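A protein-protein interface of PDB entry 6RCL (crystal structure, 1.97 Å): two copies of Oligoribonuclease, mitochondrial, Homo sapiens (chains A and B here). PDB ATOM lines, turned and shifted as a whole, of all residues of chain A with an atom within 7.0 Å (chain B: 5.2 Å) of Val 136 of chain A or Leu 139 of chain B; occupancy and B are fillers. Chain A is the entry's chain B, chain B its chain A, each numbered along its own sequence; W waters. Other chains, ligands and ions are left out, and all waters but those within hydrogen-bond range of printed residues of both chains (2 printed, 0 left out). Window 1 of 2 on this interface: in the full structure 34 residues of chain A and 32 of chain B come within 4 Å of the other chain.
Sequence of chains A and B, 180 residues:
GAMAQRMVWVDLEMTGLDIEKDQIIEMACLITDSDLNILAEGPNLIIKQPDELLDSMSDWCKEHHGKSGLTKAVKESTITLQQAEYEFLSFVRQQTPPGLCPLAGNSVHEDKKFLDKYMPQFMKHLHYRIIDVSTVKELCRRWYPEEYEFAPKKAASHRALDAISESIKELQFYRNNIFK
The side-chain hydroxyl (OG1) of Thr 135 of chain B is in hydrogen-bond range of the backbone NH (N) of Asp 132 of chain A (3.0 Å).
The indole nitrogen (NE1) of Trp 143 of chain B lies within hydrogen-bond range of the backbone carbonyl oxygen (O) of Ser 34 of chain A, 2.9 Å away.
NH1 of Arg 175 of chain A lies close to NE1 of Trp 143 of chain B (3.4 Å).
OE2 of Glu 138 of chain B is in salt-bridge range of NH2 of Arg 141 of chain B (3.1 Å).
The guanidinium group of Arg 142 of chain B is in salt-bridge range of the side-chain carboxylate of Glu 138 of chain B.
OG of Ser 134 of chain A is in hydrogen-bond range of OD1 of Asp 132 of chain A (3.0 Å).
The side-chain carboxylate (OD2) of Asp 132 of chain A lies within hydrogen-bond range of the side-chain hydroxyl (OG1) of Thr 135 of chain A (2.8 Å).
The backbone NH of Phe 179 of chain A lies within hydrogen-bond range of the backbone carbonyl oxygen of Tyr 174 of chain A (3.4 Å).
Among the printed residues, merely in contact across the chains: Phe 179 of chain A with Tyr 144 of chain B, Met 7 of chain A with Arg 142 of chain B, Ile 131 of chain A with Thr 135 of chain B, Ser 34 of chain A with Arg 142 of chain B, Leu 139 of chain A with Val 136 of chain B, Val 136 of chain A with Leu 139 of chain B, Ile 131 of chain A with Leu 139 of chain B, Leu 171 of chain A with Trp 143 of chain B and Ile 131 of chain A with Glu 138 of chain B.
Val 136 of chain A touches just one residue of chain B: Leu 139 (3.9 Å).
Of chain A, only Ile 131 and Val 136 come within 4 Å of Leu 139 of chain B.
Of the printed residues of chain B, Ser 34 of chain A touches Arg 142 (3.7 Å) and Trp 143 (2.9 Å).
Of the printed residues of chain B, Arg 175 of chain A touches Trp 143.
Arg 141 of chain B touches none of the printed residues of chain A.
Tyr 148 of chain A touches none of the printed residues of chain B.
The nearest printed residue of chain A that does not touch Leu 139 of chain B is Leu 171 of chain A (4.1 Å).
The nearest printed residue of chain A that does not touch Thr 135 of chain B is Val 136 of chain A (4.2 Å).
Hydrophobic or aromatic side chains of chain B that line the printed part of chain A: Val 136, Leu 139, Trp 143 and Tyr 144.
Printed residues of chain A that touch a printed residue of chain B: Met 7, Ser 34, Ile 131, Asp 132, Val 136, Leu 139, Leu 171, Arg 175 and Phe 179.
Hydrophobic or aromatic side chains of chain A within 4 Å of the printed part of chain B: Met 7, Ile 131, Val 136, Leu 139, Leu 171 and Phe 179.
Among the printed residues, 12 pairs touch across the chains.
Val 136 of chain A touches Leu 139 of chain B, and with the chains exchanged Leu 139 of chain A touches Val 136 of chain B.
Positions printed for both chains: 134, 135, 136, 137, 138, 139, 140, 141 and 142.
Of the 12 pairs that touch across the chains among the printed residues, 2 have their exchanged pair printed and touching as well.
Water W2 lies within hydrogen-bond range of O of Trp 143 of chain B (2.7 Å) and NH2 of Arg 175 of chain A (3.0 Å).
Water W1 lies within hydrogen-bond range of NE of Arg 175 of chain A (2.8 Å) and OH of Tyr 144 of chain B (2.9 Å).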
ATOM      1  N   MET A   7       6.732 -37.512 -18.996  1.00  0.00           N
ATOM      2  CA  MET A   7       5.414 -37.625 -18.378  1.00  0.00           C
ATOM      3  C   MET A   7       4.823 -38.954 -18.765  1.00  0.00           C
ATOM      4  O   MET A   7       4.914 -39.331 -19.930  1.00  0.00           O
ATOM      5  CB  MET A   7       4.467 -36.518 -18.876  1.00  0.00           C
ATOM      6  CG  MET A   7       5.008 -35.101 -18.761  1.00  0.00           C
ATOM      7  SD  MET A   7       3.744 -33.940 -19.350  1.00  0.00           S
ATOM      8  CE  MET A   7       4.637 -32.363 -19.148  1.00  0.00           C
ATOM      9  N   SER A  34       9.128 -33.654 -21.858  1.00  0.00           N
ATOM     10  CA  SER A  34       8.728 -32.440 -21.135  1.00  0.00           C
ATOM     11  C   SER A  34       7.877 -31.447 -21.986  1.00  0.00           C
ATOM     12  O   SER A  34       7.047 -30.718 -21.421  1.00  0.00           O
ATOM     13  CB  SER A  34       9.970 -31.738 -20.585  1.00  0.00           C
ATOM     14  OG  SER A  34      10.839 -31.287 -21.611  1.00  0.00           O
ATOM     15  N   LEU A  36       5.656 -32.375 -24.394  1.00  0.00           N
ATOM     16  CA  LEU A  36       4.457 -33.074 -24.868  1.00  0.00           C
ATOM     17  C   LEU A  36       4.613 -33.798 -26.224  1.00  0.00           C
ATOM     18  O   LEU A  36       3.597 -34.240 -26.775  1.00  0.00           O
ATOM     19  CB  LEU A  36       3.229 -32.141 -24.902  1.00  0.00           C
ATOM     20  CG  LEU A  36       3.049 -31.236 -23.668  1.00  0.00           C
ATOM     21  CD1 LEU A  36       1.774 -30.441 -23.783  1.00  0.00           C
ATOM     22  CD2 LEU A  36       3.099 -32.061 -22.382  1.00  0.00           C
ATOM     23  N   ILE A 131       0.233 -34.375 -13.301  1.00  0.00           N
ATOM     24  CA  ILE A 131       0.080 -33.264 -14.243  1.00  0.00           C
ATOM     25  C   ILE A 131      -1.362 -33.395 -14.673  1.00  0.00           C
ATOM     26  O   ILE A 131      -1.675 -34.085 -15.630  1.00  0.00           O
ATOM     27  CB  ILE A 131       1.112 -33.320 -15.414  1.00  0.00           C
ATOM     28  CG1 ILE A 131       2.527 -33.021 -14.834  1.00  0.00           C
ATOM     29  CG2 ILE A 131       0.740 -32.304 -16.552  1.00  0.00           C
ATOM     30  CD1 ILE A 131       3.640 -33.148 -15.782  1.00  0.00           C
ATOM     31  N   ASP A 132      -2.243 -32.800 -13.894  1.00  0.00           N
ATOM     32  CA  ASP A 132      -3.684 -32.850 -14.110  1.00  0.00           C
ATOM     33  C   ASP A 132      -4.098 -31.716 -15.063  1.00  0.00           C
ATOM     34  O   ASP A 132      -4.096 -30.549 -14.673  1.00  0.00           O
ATOM     35  CB  ASP A 132      -4.385 -32.744 -12.748  1.00  0.00           C
ATOM     36  CG  ASP A 132      -5.891 -32.631 -12.779  1.00  0.00           C
ATOM     37  OD1 ASP A 132      -6.514 -33.287 -13.639  1.00  0.00           O
ATOM     38  OD2 ASP A 132      -6.448 -31.866 -11.943  1.00  0.00           O
ATOM     39  N   VAL A 133      -4.496 -32.068 -16.305  1.00  0.00           N
ATOM     40  CA  VAL A 133      -4.880 -31.064 -17.286  1.00  0.00           C
ATOM     41  C   VAL A 133      -6.122 -30.302 -16.823  1.00  0.00           C
ATOM     42  O   VAL A 133      -6.226 -29.113 -17.119  1.00  0.00           O
ATOM     43  CB  VAL A 133      -5.039 -31.639 -18.729  1.00  0.00           C
ATOM     44  CG1 VAL A 133      -5.352 -30.520 -19.735  1.00  0.00           C
ATOM     45  CG2 VAL A 133      -3.779 -32.393 -19.160  1.00  0.00           C
ATOM     46  N   SER A 134      -7.039 -30.938 -16.058  1.00  0.00           N
ATOM     47  CA  SER A 134      -8.238 -30.208 -15.656  1.00  0.00           C
ATOM     48  C   SER A 134      -7.949 -29.133 -14.557  1.00  0.00           C
ATOM     49  O   SER A 134      -8.724 -28.208 -14.417  1.00  0.00           O
ATOM     50  CB  SER A 134      -9.367 -31.158 -15.287  1.00  0.00           C
ATOM     51  OG  SER A 134      -9.089 -31.836 -14.088  1.00  0.00           O
ATOM     52  N   THR A 135      -6.786 -29.177 -13.884  1.00  0.00           N
ATOM     53  CA  THR A 135      -6.389 -28.103 -12.973  1.00  0.00           C
ATOM     54  C   THR A 135      -6.129 -26.891 -13.851  1.00  0.00           C
ATOM     55  O   THR A 135      -6.649 -25.800 -13.579  1.00  0.00           O
ATOM     56  CB  THR A 135      -5.098 -28.474 -12.174  1.00  0.00           C
ATOM     57  OG1 THR A 135      -5.440 -29.397 -11.140  1.00  0.00           O
ATOM     58  CG2 THR A 135      -4.417 -27.261 -11.562  1.00  0.00           C
ATOM     59  N   VAL A 136      -5.356 -27.100 -14.941  1.00  0.00           N
ATOM     60  CA  VAL A 136      -5.010 -26.022 -15.873  1.00  0.00           C
ATOM     61  C   VAL A 136      -6.293 -25.420 -16.445  1.00  0.00           C
ATOM     62  O   VAL A 136      -6.394 -24.197 -16.553  1.00  0.00           O
ATOM     63  CB  VAL A 136      -4.022 -26.459 -17.000  1.00  0.00           C
ATOM     64  CG1 VAL A 136      -3.512 -25.231 -17.784  1.00  0.00           C
ATOM     65  CG2 VAL A 136      -2.839 -27.260 -16.440  1.00  0.00           C
ATOM     66  N   LYS A 137      -7.268 -26.258 -16.787  1.00  0.00           N
ATOM     67  CA  LYS A 137      -8.569 -25.818 -17.310  1.00  0.00           C
ATOM     68  C   LYS A 137      -9.295 -24.915 -16.291  1.00  0.00           C
ATOM     69  O   LYS A 137      -9.870 -23.893 -16.688  1.00  0.00           O
ATOM     70  CB  LYS A 137      -9.461 -27.045 -17.635  1.00  0.00           C
ATOM     71  CG  LYS A 137     -10.853 -26.669 -18.150  1.00  0.00           C
ATOM     72  CD  LYS A 137     -11.790 -27.851 -18.402  1.00  0.00           C
ATOM     73  CE  LYS A 137     -12.347 -27.889 -19.817  1.00  0.00           C
ATOM     74  NZ  LYS A 137     -13.696 -28.493 -19.865  1.00  0.00           N
ATOM     75  N   GLU A 138      -9.300 -25.308 -14.989  1.00  0.00           N
ATOM     76  CA  GLU A 138      -9.928 -24.500 -13.930  1.00  0.00           C
ATOM     77  C   GLU A 138      -9.263 -23.128 -13.799  1.00  0.00           C
ATOM     78  O   GLU A 138      -9.957 -22.167 -13.525  1.00  0.00           O
ATOM     79  CB  GLU A 138      -9.920 -25.251 -12.577  1.00  0.00           C
ATOM     80  CG  GLU A 138     -10.935 -26.386 -12.498  1.00  0.00           C
ATOM     81  CD  GLU A 138     -12.392 -25.996 -12.693  1.00  0.00           C
ATOM     82  OE1 GLU A 138     -13.114 -26.705 -13.428  1.00  0.00           O
ATOM     83  OE2 GLU A 138     -12.813 -24.974 -12.113  1.00  0.00           O
ATOM     84  N   LEU A 139      -7.935 -23.028 -14.042  1.00  0.00           N
ATOM     85  CA  LEU A 139      -7.209 -21.767 -14.026  1.00  0.00           C
ATOM     86  C   LEU A 139      -7.504 -20.985 -15.325  1.00  0.00           C
ATOM     87  O   LEU A 139      -7.717 -19.775 -15.271  1.00  0.00           O
ATOM     88  CB  LEU A 139      -5.688 -22.013 -13.842  1.00  0.00           C
ATOM     89  CG  LEU A 139      -5.260 -22.762 -12.555  1.00  0.00           C
ATOM     90  CD1 LEU A 139      -3.738 -22.861 -12.469  1.00  0.00           C
ATOM     91  CD2 LEU A 139      -5.860 -22.109 -11.276  1.00  0.00           C
ATOM     92  N   CYS A 140      -7.598 -21.671 -16.480  1.00  0.00           N
ATOM     93  CA  CYS A 140      -7.923 -20.986 -17.732  1.00  0.00           C
ATOM     94  C   CYS A 140      -9.310 -20.315 -17.656  1.00  0.00           C
ATOM     95  O   CYS A 140      -9.478 -19.159 -18.025  1.00  0.00           O
ATOM     96  CB  CYS A 140      -7.857 -21.945 -18.915  1.00  0.00           C
ATOM     97  SG  CYS A 140      -8.002 -21.115 -20.526  1.00  0.00           S
ATOM     98  N   ARG A 141     -10.276 -21.046 -17.138  1.00  0.00           N
ATOM     99  CA  ARG A 141     -11.658 -20.604 -17.014  1.00  0.00           C
ATOM    100  C   ARG A 141     -11.788 -19.308 -16.189  1.00  0.00           C
ATOM    101  O   ARG A 141     -12.612 -18.423 -16.484  1.00  0.00           O
ATOM    102  CB  ARG A 141     -12.448 -21.745 -16.330  1.00  0.00           C
ATOM    103  CG  ARG A 141     -13.936 -21.611 -16.467  1.00  0.00           C
ATOM    104  CD  ARG A 141     -14.620 -22.912 -16.094  1.00  0.00           C
ATOM    105  NE  ARG A 141     -14.434 -23.241 -14.679  1.00  0.00           N
ATOM    106  CZ  ARG A 141     -15.068 -22.652 -13.667  1.00  0.00           C
ATOM    107  NH1 ARG A 141     -15.918 -21.654 -13.890  1.00  0.00           N
ATOM    108  NH2 ARG A 141     -14.832 -23.032 -12.423  1.00  0.00           N
ATOM    109  N   ARG A 142     -10.980 -19.240 -15.120  1.00  0.00           N
ATOM    110  CA  ARG A 142     -10.962 -18.120 -14.199  1.00  0.00           C
ATOM    111  C   ARG A 142     -10.162 -16.944 -14.732  1.00  0.00           C
ATOM    112  O   ARG A 142     -10.662 -15.833 -14.756  1.00  0.00           O
ATOM    113  CB  ARG A 142     -10.342 -18.578 -12.858  1.00  0.00           C
ATOM    114  CG  ARG A 142     -11.252 -19.503 -12.046  1.00  0.00           C
ATOM    115  CD  ARG A 142     -10.577 -20.072 -10.798  1.00  0.00           C
ATOM    116  NE  ARG A 142     -11.559 -20.727  -9.922  1.00  0.00           N
ATOM    117  CZ  ARG A 142     -12.110 -21.923 -10.131  1.00  0.00           C
ATOM    118  NH1 ARG A 142     -11.787 -22.636 -11.207  1.00  0.00           N
ATOM    119  NH2 ARG A 142     -12.992 -22.416  -9.268  1.00  0.00           N
ATOM    120  N   TYR A 148     -10.569 -19.511 -22.809  1.00  0.00           N
ATOM    121  CA  TYR A 148     -11.287 -20.717 -22.424  1.00  0.00           C
ATOM    122  C   TYR A 148     -12.454 -21.013 -23.393  1.00  0.00           C
ATOM    123  O   TYR A 148     -12.657 -22.182 -23.744  1.00  0.00           O
ATOM    124  CB  TYR A 148     -11.785 -20.620 -20.963  1.00  0.00           C
ATOM    125  CG  TYR A 148     -12.660 -21.778 -20.564  1.00  0.00           C
ATOM    126  CD1 TYR A 148     -12.111 -22.956 -20.075  1.00  0.00           C
ATOM    127  CD2 TYR A 148     -14.036 -21.720 -20.723  1.00  0.00           C
ATOM    128  CE1 TYR A 148     -12.919 -24.020 -19.678  1.00  0.00           C
ATOM    129  CE2 TYR A 148     -14.853 -22.778 -20.346  1.00  0.00           C
ATOM    130  CZ  TYR A 148     -14.292 -23.925 -19.809  1.00  0.00           C
ATOM    131  OH  TYR A 148     -15.112 -24.976 -19.468  1.00  0.00           O
ATOM    132  N   GLU A 170      -5.301 -30.376 -25.548  1.00  0.00           N
ATOM    133  CA  GLU A 170      -5.858 -29.383 -24.640  1.00  0.00           C
ATOM    134  C   GLU A 170      -4.716 -28.715 -23.846  1.00  0.00           C
ATOM    135  O   GLU A 170      -4.686 -27.484 -23.741  1.00  0.00           O
ATOM    136  CB  GLU A 170      -6.886 -30.044 -23.701  1.00  0.00           C
ATOM    137  CG  GLU A 170      -7.705 -29.050 -22.891  1.00  0.00           C
ATOM    138  CD  GLU A 170      -8.625 -29.693 -21.869  1.00  0.00           C
ATOM    139  OE1 GLU A 170      -8.872 -30.916 -21.977  1.00  0.00           O
ATOM    140  OE2 GLU A 170      -9.088 -28.980 -20.952  1.00  0.00           O
ATOM    141  N   LEU A 171      -3.771 -29.515 -23.299  1.00  0.00           N
ATOM    142  CA  LEU A 171      -2.651 -28.959 -22.525  1.00  0.00           C
ATOM    143  C   LEU A 171      -1.714 -28.080 -23.388  1.00  0.00           C
ATOM    144  O   LEU A 171      -1.251 -27.035 -22.929  1.00  0.00           O
ATOM    145  CB  LEU A 171      -1.844 -30.063 -21.816  1.00  0.00           C
ATOM    146  CG  LEU A 171      -0.680 -29.588 -20.919  1.00  0.00           C
ATOM    147  CD1 LEU A 171      -1.168 -28.601 -19.800  1.00  0.00           C
ATOM    148  CD2 LEU A 171       0.059 -30.775 -20.306  1.00  0.00           C
ATOM    149  N   TYR A 174      -3.315 -24.721 -23.745  1.00  0.00           N
ATOM    150  CA  TYR A 174      -3.093 -23.812 -22.626  1.00  0.00           C
ATOM    151  C   TYR A 174      -1.667 -23.336 -22.661  1.00  0.00           C
ATOM    152  O   TYR A 174      -1.467 -22.151 -22.454  1.00  0.00           O
ATOM    153  CB  TYR A 174      -3.423 -24.459 -21.247  1.00  0.00           C
ATOM    154  CG  TYR A 174      -4.848 -24.944 -21.162  1.00  0.00           C
ATOM    155  CD1 TYR A 174      -5.908 -24.094 -21.435  1.00  0.00           C
ATOM    156  CD2 TYR A 174      -5.143 -26.230 -20.711  1.00  0.00           C
ATOM    157  CE1 TYR A 174      -7.221 -24.555 -21.426  1.00  0.00           C
ATOM    158  CE2 TYR A 174      -6.456 -26.654 -20.558  1.00  0.00           C
ATOM    159  CZ  TYR A 174      -7.493 -25.838 -20.974  1.00  0.00           C
ATOM    160  OH  TYR A 174      -8.776 -26.323 -20.953  1.00  0.00           O
ATOM    161  N   ARG A 175      -0.665 -24.203 -22.990  1.00  0.00           N
ATOM    162  CA  ARG A 175       0.712 -23.675 -23.048  1.00  0.00           C
ATOM    163  C   ARG A 175       0.815 -22.443 -23.992  1.00  0.00           C
ATOM    164  O   ARG A 175       1.399 -21.424 -23.629  1.00  0.00           O
ATOM    165  CB  ARG A 175       1.712 -24.727 -23.503  1.00  0.00           C
ATOM    166  CG  ARG A 175       3.149 -24.240 -23.314  1.00  0.00           C
ATOM    167  CD  ARG A 175       4.178 -25.276 -23.681  1.00  0.00           C
ATOM    168  NE  ARG A 175       5.523 -24.721 -23.503  1.00  0.00           N
ATOM    169  CZ  ARG A 175       6.659 -25.398 -23.658  1.00  0.00           C
ATOM    170  NH1 ARG A 175       6.637 -26.677 -24.020  1.00  0.00           N
ATOM    171  NH2 ARG A 175       7.830 -24.800 -23.449  1.00  0.00           N
ATOM    172  N   ILE A 178      -2.282 -19.339 -22.645  1.00  0.00           N
ATOM    173  CA  ILE A 178      -2.350 -18.662 -21.332  1.00  0.00           C
ATOM    174  C   ILE A 178      -1.037 -18.616 -20.580  1.00  0.00           C
ATOM    175  O   ILE A 178      -0.948 -17.833 -19.619  1.00  0.00           O
ATOM    176  CB  ILE A 178      -3.463 -19.290 -20.469  1.00  0.00           C
ATOM    177  CG1 ILE A 178      -3.134 -20.723 -20.021  1.00  0.00           C
ATOM    178  CG2 ILE A 178      -4.812 -19.247 -21.229  1.00  0.00           C
ATOM    179  CD1 ILE A 178      -4.054 -21.161 -18.834  1.00  0.00           C
ATOM    180  N   PHE A 179      -0.025 -19.421 -20.975  1.00  0.00           N
ATOM    181  CA  PHE A 179       1.281 -19.363 -20.308  1.00  0.00           C
ATOM    182  C   PHE A 179       2.105 -18.304 -21.051  1.00  0.00           C
ATOM    183  O   PHE A 179       1.827 -18.004 -22.219  1.00  0.00           O
ATOM    184  CB  PHE A 179       1.979 -20.739 -20.238  1.00  0.00           C
ATOM    185  CG  PHE A 179       1.404 -21.683 -19.198  1.00  0.00           C
ATOM    186  CD1 PHE A 179       2.028 -21.854 -17.962  1.00  0.00           C
ATOM    187  CD2 PHE A 179       0.264 -22.434 -19.471  1.00  0.00           C
ATOM    188  CE1 PHE A 179       1.528 -22.767 -17.039  1.00  0.00           C
ATOM    189  CE2 PHE A 179      -0.230 -23.353 -18.538  1.00  0.00           C
ATOM    190  CZ  PHE A 179       0.395 -23.513 -17.341  1.00  0.00           C
ATOM    191  N   SER B 134       0.724 -28.461  -7.488  1.00  0.00           N
ATOM    192  CA  SER B 134       1.903 -29.260  -7.883  1.00  0.00           C
ATOM    193  C   SER B 134       1.890 -29.667  -9.365  1.00  0.00           C
ATOM    194  O   SER B 134       2.947 -29.979  -9.908  1.00  0.00           O
ATOM    195  CB  SER B 134       2.110 -30.455  -6.970  1.00  0.00           C
ATOM    196  OG  SER B 134       2.309 -29.950  -5.660  1.00  0.00           O
ATOM    197  N   THR B 135       0.725 -29.612 -10.033  1.00  0.00           N
ATOM    198  CA  THR B 135       0.666 -29.760 -11.483  1.00  0.00           C
ATOM    199  C   THR B 135       1.349 -28.535 -12.097  1.00  0.00           C
ATOM    200  O   THR B 135       2.142 -28.686 -13.018  1.00  0.00           O
ATOM    201  CB  THR B 135      -0.792 -29.751 -12.011  1.00  0.00           C
ATOM    202  OG1 THR B 135      -1.386 -31.000 -11.712  1.00  0.00           O
ATOM    203  CG2 THR B 135      -0.864 -29.502 -13.548  1.00  0.00           C
ATOM    204  N   VAL B 136       1.018 -27.317 -11.586  1.00  0.00           N
ATOM    205  CA  VAL B 136       1.591 -26.069 -12.099  1.00  0.00           C
ATOM    206  C   VAL B 136       3.088 -26.023 -11.789  1.00  0.00           C
ATOM    207  O   VAL B 136       3.857 -25.600 -12.644  1.00  0.00           O
ATOM    208  CB  VAL B 136       0.852 -24.810 -11.603  1.00  0.00           C
ATOM    209  CG1 VAL B 136       1.329 -23.563 -12.374  1.00  0.00           C
ATOM    210  CG2 VAL B 136      -0.678 -24.986 -11.740  1.00  0.00           C
ATOM    211  N   LYS B 137       3.499 -26.523 -10.602  1.00  0.00           N
ATOM    212  CA  LYS B 137       4.903 -26.652 -10.234  1.00  0.00           C
ATOM    213  C   LYS B 137       5.632 -27.510 -11.279  1.00  0.00           C
ATOM    214  O   LYS B 137       6.636 -27.072 -11.833  1.00  0.00           O
ATOM    215  CB  LYS B 137       5.036 -27.321  -8.862  1.00  0.00           C
ATOM    216  CG  LYS B 137       6.484 -27.531  -8.374  1.00  0.00           C
ATOM    217  CD  LYS B 137       6.584 -28.709  -7.396  1.00  0.00           C
ATOM    218  CE  LYS B 137       5.787 -28.529  -6.103  1.00  0.00           C
ATOM    219  NZ  LYS B 137       6.322 -27.445  -5.238  1.00  0.00           N
ATOM    220  N   GLU B 138       5.112 -28.708 -11.552  1.00  0.00           N
ATOM    221  CA  GLU B 138       5.736 -29.623 -12.514  1.00  0.00           C
ATOM    222  C   GLU B 138       5.807 -29.027 -13.927  1.00  0.00           C
ATOM    223  O   GLU B 138       6.811 -29.236 -14.603  1.00  0.00           O
ATOM    224  CB  GLU B 138       5.049 -31.016 -12.490  1.00  0.00           C
ATOM    225  CG  GLU B 138       5.413 -31.858 -11.268  1.00  0.00           C
ATOM    226  CD  GLU B 138       6.901 -31.946 -11.000  1.00  0.00           C
ATOM    227  OE1 GLU B 138       7.665 -32.176 -11.967  1.00  0.00           O
ATOM    228  OE2 GLU B 138       7.313 -31.737  -9.838  1.00  0.00           O
ATOM    229  N   LEU B 139       4.813 -28.224 -14.339  1.00  0.00           N
ATOM    230  CA  LEU B 139       4.864 -27.553 -15.635  1.00  0.00           C
ATOM    231  C   LEU B 139       5.871 -26.399 -15.579  1.00  0.00           C
ATOM    232  O   LEU B 139       6.595 -26.166 -16.558  1.00  0.00           O
ATOM    233  CB  LEU B 139       3.479 -27.045 -16.061  1.00  0.00           C
ATOM    234  CG  LEU B 139       2.406 -28.128 -16.264  1.00  0.00           C
ATOM    235  CD1 LEU B 139       1.031 -27.501 -16.512  1.00  0.00           C
ATOM    236  CD2 LEU B 139       2.787 -29.094 -17.352  1.00  0.00           C
ATOM    237  N   CYS B 140       5.964 -25.701 -14.430  1.00  0.00           N
ATOM    238  CA  CYS B 140       6.934 -24.596 -14.284  1.00  0.00           C
ATOM    239  C   CYS B 140       8.364 -25.114 -14.418  1.00  0.00           C
ATOM    240  O   CYS B 140       9.159 -24.536 -15.149  1.00  0.00           O
ATOM    241  CB  CYS B 140       6.753 -23.862 -12.960  1.00  0.00           C
ATOM    242  SG  CYS B 140       7.784 -22.380 -12.811  1.00  0.00           S
ATOM    243  N   ARG B 141       8.678 -26.199 -13.695  1.00  0.00           N
ATOM    244  CA  ARG B 141       9.986 -26.859 -13.699  1.00  0.00           C
ATOM    245  C   ARG B 141      10.431 -27.158 -15.112  1.00  0.00           C
ATOM    246  O   ARG B 141      11.595 -26.948 -15.442  1.00  0.00           O
ATOM    247  CB  ARG B 141       9.908 -28.181 -12.911  1.00  0.00           C
ATOM    248  CG  ARG B 141      11.208 -29.006 -12.895  1.00  0.00           C
ATOM    249  CD  ARG B 141      10.959 -30.426 -12.437  1.00  0.00           C
ATOM    250  NE  ARG B 141      10.171 -30.439 -11.209  1.00  0.00           N
ATOM    251  CZ  ARG B 141      10.639 -30.200  -9.986  1.00  0.00           C
ATOM    252  NH1 ARG B 141      11.934 -29.953  -9.792  1.00  0.00           N
ATOM    253  NH2 ARG B 141       9.821 -30.213  -8.943  1.00  0.00           N
ATOM    254  N   ARG B 142       9.519 -27.719 -15.919  1.00  0.00           N
ATOM    255  CA  ARG B 142       9.784 -28.058 -17.332  1.00  0.00           C
ATOM    256  C   ARG B 142       9.842 -26.872 -18.305  1.00  0.00           C
ATOM    257  O   ARG B 142      10.809 -26.733 -19.065  1.00  0.00           O
ATOM    258  CB  ARG B 142       8.716 -29.039 -17.842  1.00  0.00           C
ATOM    259  CG  ARG B 142       8.886 -30.410 -17.256  1.00  0.00           C
ATOM    260  CD  ARG B 142       7.647 -31.247 -17.486  1.00  0.00           C
ATOM    261  NE  ARG B 142       7.813 -32.603 -16.961  1.00  0.00           N
ATOM    262  CZ  ARG B 142       7.807 -32.947 -15.673  1.00  0.00           C
ATOM    263  NH1 ARG B 142       7.631 -32.026 -14.727  1.00  0.00           N
ATOM    264  NH2 ARG B 142       7.967 -34.212 -15.320  1.00  0.00           N
ATOM    265  N   TRP B 143       8.776 -26.078 -18.362  1.00  0.00           N
ATOM    266  CA  TRP B 143       8.650 -25.009 -19.360  1.00  0.00           C
ATOM    267  C   TRP B 143       9.236 -23.664 -19.014  1.00  0.00           C
ATOM    268  O   TRP B 143       9.486 -22.874 -19.939  1.00  0.00           O
ATOM    269  CB  TRP B 143       7.178 -24.787 -19.722  1.00  0.00           C
ATOM    270  CG  TRP B 143       6.448 -26.026 -20.158  1.00  0.00           C
ATOM    271  CD1 TRP B 143       6.987 -27.167 -20.682  1.00  0.00           C
ATOM    272  CD2 TRP B 143       5.017 -26.206 -20.179  1.00  0.00           C
ATOM    273  NE1 TRP B 143       5.989 -28.073 -20.962  1.00  0.00           N
ATOM    274  CE2 TRP B 143       4.768 -27.493 -20.704  1.00  0.00           C
ATOM    275  CE3 TRP B 143       3.927 -25.396 -19.805  1.00  0.00           C
ATOM    276  CZ2 TRP B 143       3.464 -27.981 -20.901  1.00  0.00           C
ATOM    277  CZ3 TRP B 143       2.642 -25.885 -19.968  1.00  0.00           C
ATOM    278  CH2 TRP B 143       2.417 -27.173 -20.484  1.00  0.00           C
ATOM    279  N   TYR B 144       9.382 -23.362 -17.704  1.00  0.00           N
ATOM    280  CA  TYR B 144       9.876 -22.075 -17.204  1.00  0.00           C
ATOM    281  C   TYR B 144      10.981 -22.325 -16.178  1.00  0.00           C
ATOM    282  O   TYR B 144      10.853 -21.904 -15.029  1.00  0.00           O
ATOM    283  CB  TYR B 144       8.688 -21.303 -16.590  1.00  0.00           C
ATOM    284  CG  TYR B 144       7.701 -20.929 -17.663  1.00  0.00           C
ATOM    285  CD1 TYR B 144       7.944 -19.848 -18.511  1.00  0.00           C
ATOM    286  CD2 TYR B 144       6.588 -21.726 -17.924  1.00  0.00           C
ATOM    287  CE1 TYR B 144       7.097 -19.558 -19.577  1.00  0.00           C
ATOM    288  CE2 TYR B 144       5.741 -21.453 -19.001  1.00  0.00           C
ATOM    289  CZ  TYR B 144       5.998 -20.366 -19.823  1.00  0.00           C
ATOM    290  OH  TYR B 144       5.210 -20.141 -20.936  1.00  0.00           O
HETATM  291  O   HOH W   1       5.922 -22.046 -22.973  1.00  0.00           O
HETATM  292  O   HOH W   2       8.507 -22.117 -22.377  1.00  0.00           O
